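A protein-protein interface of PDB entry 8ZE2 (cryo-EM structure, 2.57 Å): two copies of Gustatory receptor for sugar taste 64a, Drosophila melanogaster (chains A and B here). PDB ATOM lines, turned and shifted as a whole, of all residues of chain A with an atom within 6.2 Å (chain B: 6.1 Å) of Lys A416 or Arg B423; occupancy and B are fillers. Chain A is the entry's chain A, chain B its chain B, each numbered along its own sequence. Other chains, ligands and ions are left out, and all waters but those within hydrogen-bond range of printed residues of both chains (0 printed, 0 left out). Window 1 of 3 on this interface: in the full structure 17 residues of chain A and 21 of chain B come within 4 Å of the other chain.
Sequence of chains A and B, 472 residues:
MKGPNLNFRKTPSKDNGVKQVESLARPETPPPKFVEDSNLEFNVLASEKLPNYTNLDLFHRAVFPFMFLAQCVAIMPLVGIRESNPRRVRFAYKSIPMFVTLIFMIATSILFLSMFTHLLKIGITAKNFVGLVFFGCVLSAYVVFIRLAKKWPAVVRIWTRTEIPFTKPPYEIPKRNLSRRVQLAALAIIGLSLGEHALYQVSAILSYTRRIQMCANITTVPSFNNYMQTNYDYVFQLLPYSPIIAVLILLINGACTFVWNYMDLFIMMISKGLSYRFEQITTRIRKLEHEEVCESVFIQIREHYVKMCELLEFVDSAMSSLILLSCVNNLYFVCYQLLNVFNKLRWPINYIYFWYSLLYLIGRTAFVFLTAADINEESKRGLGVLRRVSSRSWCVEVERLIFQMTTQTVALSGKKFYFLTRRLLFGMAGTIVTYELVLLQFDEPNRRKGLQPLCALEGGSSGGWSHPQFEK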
ATOM      1  N   GLU A 313      -9.247  19.017 -11.231  1.00  0.00           N
ATOM      2  CA  GLU A 313      -8.055  19.758 -10.826  1.00  0.00           C
ATOM      3  C   GLU A 313      -8.410  21.151 -10.320  1.00  0.00           C
ATOM      4  O   GLU A 313      -7.846  21.619  -9.325  1.00  0.00           O
ATOM      5  CB  GLU A 313      -7.064  19.850 -11.987  1.00  0.00           C
ATOM      6  CG  GLU A 313      -6.366  18.544 -12.324  1.00  0.00           C
ATOM      7  CD  GLU A 313      -5.506  18.645 -13.570  1.00  0.00           C
ATOM      8  OE1 GLU A 313      -5.285  19.775 -14.056  1.00  0.00           O
ATOM      9  OE2 GLU A 313      -5.044  17.593 -14.059  1.00  0.00           O
ATOM     10  N   ASP A 316      -9.997  20.753  -7.017  1.00  0.00           N
ATOM     11  CA  ASP A 316      -8.967  20.388  -6.053  1.00  0.00           C
ATOM     12  C   ASP A 316      -8.153  21.603  -5.634  1.00  0.00           C
ATOM     13  O   ASP A 316      -7.831  21.760  -4.455  1.00  0.00           O
ATOM     14  CB  ASP A 316      -8.062  19.306  -6.640  1.00  0.00           C
ATOM     15  CG  ASP A 316      -7.896  18.124  -5.709  1.00  0.00           C
ATOM     16  OD1 ASP A 316      -8.295  18.244  -4.532  1.00  0.00           O
ATOM     17  OD2 ASP A 316      -7.366  17.083  -6.148  1.00  0.00           O
ATOM     18  N   ALA A 411      -8.177  11.638  -9.079  1.00  0.00           N
ATOM     19  CA  ALA A 411      -8.904  11.588  -7.816  1.00  0.00           C
ATOM     20  C   ALA A 411      -8.718  12.915  -7.096  1.00  0.00           C
ATOM     21  O   ALA A 411      -7.840  13.712  -7.437  1.00  0.00           O
ATOM     22  CB  ALA A 411      -8.430  10.426  -6.939  1.00  0.00           C
ATOM     23  N   SER A 413      -7.517  15.235  -4.005  1.00  0.00           N
ATOM     24  CA  SER A 413      -6.290  15.226  -3.225  1.00  0.00           C
ATOM     25  C   SER A 413      -6.369  16.302  -2.153  1.00  0.00           C
ATOM     26  O   SER A 413      -7.133  17.263  -2.265  1.00  0.00           O
ATOM     27  CB  SER A 413      -5.057  15.448  -4.110  1.00  0.00           C
ATOM     28  OG  SER A 413      -5.102  16.719  -4.734  1.00  0.00           O
ATOM     29  N   GLY A 414      -5.575  16.125  -1.101  1.00  0.00           N
ATOM     30  CA  GLY A 414      -5.500  17.144  -0.076  1.00  0.00           C
ATOM     31  C   GLY A 414      -4.799  18.384  -0.590  1.00  0.00           C
ATOM     32  O   GLY A 414      -5.444  19.400  -0.861  1.00  0.00           O
ATOM     33  N   LYS A 415      -3.479  18.311  -0.734  1.00  0.00           N
ATOM     34  CA  LYS A 415      -2.697  19.310  -1.458  1.00  0.00           C
ATOM     35  C   LYS A 415      -1.622  18.623  -2.283  1.00  0.00           C
ATOM     36  O   LYS A 415      -0.464  19.050  -2.305  1.00  0.00           O
ATOM     37  CB  LYS A 415      -2.078  20.339  -0.513  1.00  0.00           C
ATOM     38  CG  LYS A 415      -2.780  21.685  -0.533  1.00  0.00           C
ATOM     39  CD  LYS A 415      -2.051  22.717   0.311  1.00  0.00           C
ATOM     40  CE  LYS A 415      -2.827  24.025   0.366  1.00  0.00           C
ATOM     41  NZ  LYS A 415      -2.915  24.680  -0.969  1.00  0.00           N
ATOM     42  N   LYS A 416      -1.996  17.534  -2.955  1.00  0.00           N
ATOM     43  CA  LYS A 416      -1.132  16.583  -3.649  1.00  0.00           C
ATOM     44  C   LYS A 416      -0.328  15.761  -2.647  1.00  0.00           C
ATOM     45  O   LYS A 416       0.503  14.946  -3.065  1.00  0.00           O
ATOM     46  CB  LYS A 416      -0.177  17.242  -4.659  1.00  0.00           C
ATOM     47  CG  LYS A 416      -0.886  18.028  -5.749  1.00  0.00           C
ATOM     48  CD  LYS A 416      -1.223  17.143  -6.936  1.00  0.00           C
ATOM     49  CE  LYS A 416      -2.291  17.777  -7.811  1.00  0.00           C
ATOM     50  NZ  LYS A 416      -3.663  17.455  -7.331  1.00  0.00           N
ATOM     51  N   PHE A 417      -0.543  15.947  -1.342  1.00  0.00           N
ATOM     52  CA  PHE A 417       0.094  15.088  -0.351  1.00  0.00           C
ATOM     53  C   PHE A 417      -0.432  13.663  -0.435  1.00  0.00           C
ATOM     54  O   PHE A 417       0.306  12.709  -0.166  1.00  0.00           O
ATOM     55  CB  PHE A 417      -0.133  15.646   1.054  1.00  0.00           C
ATOM     56  CG  PHE A 417       0.623  16.911   1.338  1.00  0.00           C
ATOM     57  CD1 PHE A 417       1.918  17.080   0.879  1.00  0.00           C
ATOM     58  CD2 PHE A 417       0.037  17.930   2.069  1.00  0.00           C
ATOM     59  CE1 PHE A 417       2.614  18.244   1.143  1.00  0.00           C
ATOM     60  CE2 PHE A 417       0.728  19.096   2.336  1.00  0.00           C
ATOM     61  CZ  PHE A 417       2.017  19.253   1.872  1.00  0.00           C
ATOM     62  N   TYR A 418      -1.703  13.501  -0.794  1.00  0.00           N
ATOM     63  CA  TYR A 418      -2.329  12.192  -0.904  1.00  0.00           C
ATOM     64  C   TYR A 418      -3.549  12.318  -1.802  1.00  0.00           C
ATOM     65  O   TYR A 418      -4.266  13.319  -1.753  1.00  0.00           O
ATOM     66  CB  TYR A 418      -2.722  11.644   0.473  1.00  0.00           C
ATOM     67  CG  TYR A 418      -3.462  12.640   1.341  1.00  0.00           C
ATOM     68  CD1 TYR A 418      -4.839  12.792   1.245  1.00  0.00           C
ATOM     69  CD2 TYR A 418      -2.780  13.431   2.255  1.00  0.00           C
ATOM     70  CE1 TYR A 418      -5.514  13.701   2.035  1.00  0.00           C
ATOM     71  CE2 TYR A 418      -3.446  14.340   3.049  1.00  0.00           C
ATOM     72  CZ  TYR A 418      -4.812  14.472   2.937  1.00  0.00           C
ATOM     73  OH  TYR A 418      -5.476  15.379   3.727  1.00  0.00           O
ATOM     74  N   PHE A 419      -3.776  11.295  -2.619  1.00  0.00           N
ATOM     75  CA  PHE A 419      -4.895  11.261  -3.550  1.00  0.00           C
ATOM     76  C   PHE A 419      -5.981  10.351  -2.996  1.00  0.00           C
ATOM     77  O   PHE A 419      -5.723   9.179  -2.707  1.00  0.00           O
ATOM     78  CB  PHE A 419      -4.448  10.777  -4.930  1.00  0.00           C
ATOM     79  CG  PHE A 419      -3.683  11.803  -5.714  1.00  0.00           C
ATOM     80  CD1 PHE A 419      -2.361  12.082  -5.411  1.00  0.00           C
ATOM     81  CD2 PHE A 419      -4.286  12.490  -6.755  1.00  0.00           C
ATOM     82  CE1 PHE A 419      -1.654  13.025  -6.131  1.00  0.00           C
ATOM     83  CE2 PHE A 419      -3.585  13.434  -7.479  1.00  0.00           C
ATOM     84  CZ  PHE A 419      -2.267  13.702  -7.166  1.00  0.00           C
ATOM     85  N   LEU A 424      -5.894   4.698  -0.804  1.00  0.00           N
ATOM     86  CA  LEU A 424      -5.675   5.638   0.289  1.00  0.00           C
ATOM     87  C   LEU A 424      -6.611   5.357   1.455  1.00  0.00           C
ATOM     88  O   LEU A 424      -6.226   5.551   2.609  1.00  0.00           O
ATOM     89  CB  LEU A 424      -5.848   7.081  -0.190  1.00  0.00           C
ATOM     90  CG  LEU A 424      -5.784   8.138   0.923  1.00  0.00           C
ATOM     91  CD1 LEU A 424      -4.480   8.024   1.707  1.00  0.00           C
ATOM     92  CD2 LEU A 424      -5.960   9.546   0.395  1.00  0.00           C
ATOM     93  N   GLU B 377       6.506  18.790  -8.729  1.00  0.00           N
ATOM     94  CA  GLU B 377       5.172  19.324  -8.968  1.00  0.00           C
ATOM     95  C   GLU B 377       5.131  20.192 -10.215  1.00  0.00           C
ATOM     96  O   GLU B 377       4.136  20.180 -10.940  1.00  0.00           O
ATOM     97  CB  GLU B 377       4.691  20.121  -7.756  1.00  0.00           C
ATOM     98  CG  GLU B 377       4.661  19.331  -6.463  1.00  0.00           C
ATOM     99  CD  GLU B 377       3.874  18.042  -6.582  1.00  0.00           C
ATOM    100  OE1 GLU B 377       2.726  18.088  -7.073  1.00  0.00           O
ATOM    101  OE2 GLU B 377       4.400  16.984  -6.180  1.00  0.00           O
ATOM    102  N   LYS B 380       5.238  17.975 -13.204  1.00  0.00           N
ATOM    103  CA  LYS B 380       3.944  17.323 -13.360  1.00  0.00           C
ATOM    104  C   LYS B 380       2.832  18.291 -13.751  1.00  0.00           C
ATOM    105  O   LYS B 380       1.814  17.855 -14.295  1.00  0.00           O
ATOM    106  CB  LYS B 380       3.565  16.603 -12.064  1.00  0.00           C
ATOM    107  CG  LYS B 380       4.228  15.243 -11.892  1.00  0.00           C
ATOM    108  CD  LYS B 380       4.459  14.907 -10.424  1.00  0.00           C
ATOM    109  CE  LYS B 380       3.297  15.354  -9.550  1.00  0.00           C
ATOM    110  NZ  LYS B 380       3.534  15.040  -8.114  1.00  0.00           N
ATOM    111  N   THR B 421       9.537  14.753  -2.845  1.00  0.00           N
ATOM    112  CA  THR B 421       8.258  15.043  -3.476  1.00  0.00           C
ATOM    113  C   THR B 421       7.246  15.386  -2.393  1.00  0.00           C
ATOM    114  O   THR B 421       7.492  15.192  -1.199  1.00  0.00           O
ATOM    115  CB  THR B 421       7.756  13.858  -4.314  1.00  0.00           C
ATOM    116  OG1 THR B 421       7.750  12.671  -3.512  1.00  0.00           O
ATOM    117  CG2 THR B 421       8.651  13.637  -5.524  1.00  0.00           C
ATOM    118  N   ARG B 422       6.094  15.914  -2.818  1.00  0.00           N
ATOM    119  CA  ARG B 422       5.004  16.145  -1.874  1.00  0.00           C
ATOM    120  C   ARG B 422       4.532  14.832  -1.264  1.00  0.00           C
ATOM    121  O   ARG B 422       4.161  14.782  -0.085  1.00  0.00           O
ATOM    122  CB  ARG B 422       3.843  16.865  -2.560  1.00  0.00           C
ATOM    123  CG  ARG B 422       4.101  18.333  -2.856  1.00  0.00           C
ATOM    124  CD  ARG B 422       2.858  19.002  -3.426  1.00  0.00           C
ATOM    125  NE  ARG B 422       2.783  20.416  -3.081  1.00  0.00           N
ATOM    126  CZ  ARG B 422       2.134  20.899  -2.030  1.00  0.00           C
ATOM    127  NH1 ARG B 422       1.482  20.106  -1.196  1.00  0.00           N
ATOM    128  NH2 ARG B 422       2.139  22.211  -1.812  1.00  0.00           N
ATOM    129  N   ARG B 423       4.540  13.757  -2.055  1.00  0.00           N
ATOM    130  CA  ARG B 423       4.285  12.431  -1.503  1.00  0.00           C
ATOM    131  C   ARG B 423       5.317  12.080  -0.442  1.00  0.00           C
ATOM    132  O   ARG B 423       4.971  11.559   0.625  1.00  0.00           O
ATOM    133  CB  ARG B 423       4.283  11.386  -2.617  1.00  0.00           C
ATOM    134  CG  ARG B 423       2.994  11.319  -3.417  1.00  0.00           C
ATOM    135  CD  ARG B 423       1.786  11.239  -2.500  1.00  0.00           C
ATOM    136  NE  ARG B 423       1.450   9.863  -2.154  1.00  0.00           N
ATOM    137  CZ  ARG B 423       1.222   9.437  -0.919  1.00  0.00           C
ATOM    138  NH1 ARG B 423       1.289  10.254   0.117  1.00  0.00           N
ATOM    139  NH2 ARG B 423       0.922   8.157  -0.721  1.00  0.00           N
ATOM    140  N   LEU B 424       6.594  12.370  -0.710  1.00  0.00           N
ATOM    141  CA  LEU B 424       7.620  12.129   0.297  1.00  0.00           C
ATOM    142  C   LEU B 424       7.442  13.048   1.497  1.00  0.00           C
ATOM    143  O   LEU B 424       7.728  12.643   2.625  1.00  0.00           O
ATOM    144  CB  LEU B 424       9.019  12.304  -0.296  1.00  0.00           C
ATOM    145  CG  LEU B 424      10.164  12.217   0.723  1.00  0.00           C
ATOM    146  CD1 LEU B 424      10.107  10.901   1.495  1.00  0.00           C
ATOM    147  CD2 LEU B 424      11.526  12.395   0.084  1.00  0.00           C
ATOM    148  N   LEU B 425       6.976  14.281   1.286  1.00  0.00           N
ATOM    149  CA  LEU B 425       6.734  15.164   2.423  1.00  0.00           C
ATOM    150  C   LEU B 425       5.625  14.621   3.317  1.00  0.00           C
ATOM    151  O   LEU B 425       5.741  14.655   4.548  1.00  0.00           O
ATOM    152  CB  LEU B 425       6.394  16.574   1.944  1.00  0.00           C
ATOM    153  CG  LEU B 425       6.217  17.594   3.072  1.00  0.00           C
ATOM    154  CD1 LEU B 425       7.426  17.595   3.999  1.00  0.00           C
ATOM    155  CD2 LEU B 425       5.968  18.981   2.515  1.00  0.00           C
ATOM    156  N   PHE B 426       4.545  14.112   2.721  1.00  0.00           N
ATOM    157  CA  PHE B 426       3.482  13.515   3.523  1.00  0.00           C
ATOM    158  C   PHE B 426       3.957  12.242   4.212  1.00  0.00           C
ATOM    159  O   PHE B 426       3.595  11.979   5.367  1.00  0.00           O
ATOM    160  CB  PHE B 426       2.257  13.226   2.657  1.00  0.00           C
ATOM    161  CG  PHE B 426       1.096  12.665   3.424  1.00  0.00           C
ATOM    162  CD1 PHE B 426       0.730  13.210   4.645  1.00  0.00           C
ATOM    163  CD2 PHE B 426       0.382  11.585   2.937  1.00  0.00           C
ATOM    164  CE1 PHE B 426      -0.333  12.695   5.359  1.00  0.00           C
ATOM    165  CE2 PHE B 426      -0.682  11.063   3.648  1.00  0.00           C
ATOM    166  CZ  PHE B 426      -1.040  11.620   4.861  1.00  0.00           C
ATOM    167  N   GLY B 427       4.759  11.433   3.517  1.00  0.00           N
ATOM    168  CA  GLY B 427       5.328  10.254   4.149  1.00  0.00           C
ATOM    169  C   GLY B 427       6.231  10.607   5.313  1.00  0.00           C
ATOM    170  O   GLY B 427       6.228   9.929   6.340  1.00  0.00           O
ATOM    171  N   MET B 428       7.011  11.679   5.168  1.00  0.00           N
ATOM    172  CA  MET B 428       7.841  12.167   6.262  1.00  0.00           C
ATOM    173  C   MET B 428       6.989  12.657   7.422  1.00  0.00           C
ATOM    174  O   MET B 428       7.331  12.431   8.584  1.00  0.00           O
ATOM    175  CB  MET B 428       8.755  13.286   5.767  1.00  0.00           C
ATOM    176  CG  MET B 428       9.807  13.709   6.773  1.00  0.00           C
ATOM    177  SD  MET B 428      10.794  15.092   6.181  1.00  0.00           S
ATOM    178  CE  MET B 428      11.857  15.381   7.591  1.00  0.00           C
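1 position is printed for both chains.
Of the 9 pairs that touch across the chains among the printed residues, none has its exchanged pair printed and touching as well.
Hydrophobic or aromatic side chains of chain B within 4 Å of the printed part of chain A: Leu B425 and Phe B426.
Printed residues of chain A that touch a printed residue of chain B: Lys A415, Lys A416, Phe A417 and Tyr A418.
Hydrophobic or aromatic side chains of chain A that line the printed part of chain B: Phe A417 and Tyr A418.
Among the printed residues, 9 pairs touch across the chains.
Among the printed residues, no Asp or Glu carboxylate lies within 4 Å of a Lys or Arg side-chain nitrogen of the other chain.
Glu B377 touches Lys A416.
CB of Lys A416 touches CD of Arg B422 (3.7 Å).
Lys A416 touches Arg B423 (O to CD, 3.96 Å).
NH1 of Arg B422 touches CE1 of Phe A417 (3.2 Å).
CE1 of Phe A417 touches CD2 of Leu B425 (3.7 Å).
O of Phe A417 touches CD2 of Phe B426, 3.3 Å away.
Tyr A418 touches Phe B426 (CD2 to CE2, 3.5 Å).
NH1 of Arg B422 lies within hydrogen-bond range of O of Lys A415, 2.5 Å away.
O of Phe A417 is in hydrogen-bond range of NH1 of Arg B423 (2.7 Å).
Of the printed residues of chain B, Lys A416 touches Glu B377, Arg B422 and Arg B423.
Of the printed residues of chain A, Arg B423 touches Lys A416 (3.96 Å) and Phe A417 (2.7 Å).
Printed residues of chain A within 4 Å of Glu B377: Lys A416 (3.8 Å).
Of the printed residues of chain A, Phe B426 touches Phe A417 (3.3 Å) and Tyr A418 (3.5 Å).
Thr B421 touches none of the printed residues of chain A.
Ala A411 touches none of the printed residues of chain B.
The nearest residue of chain B that does not touch Lys A416 is Lys B380 (5.3 Å).
The nearest printed residue of chain A that does not touch Leu B425 is Lys A416 (7.8 Å).
The side-chain carboxylate (OD2) of Asp A316 lies within salt-bridge range of the side-chain amino group (NZ) of Lys A416 (3.9 Å).
NZ of Lys A416 lies within hydrogen-bond range of OG of Ser A413.
NZ of Lys B380 lies within salt-bridge range of OE2 of Glu B377, at 2.9 Å.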
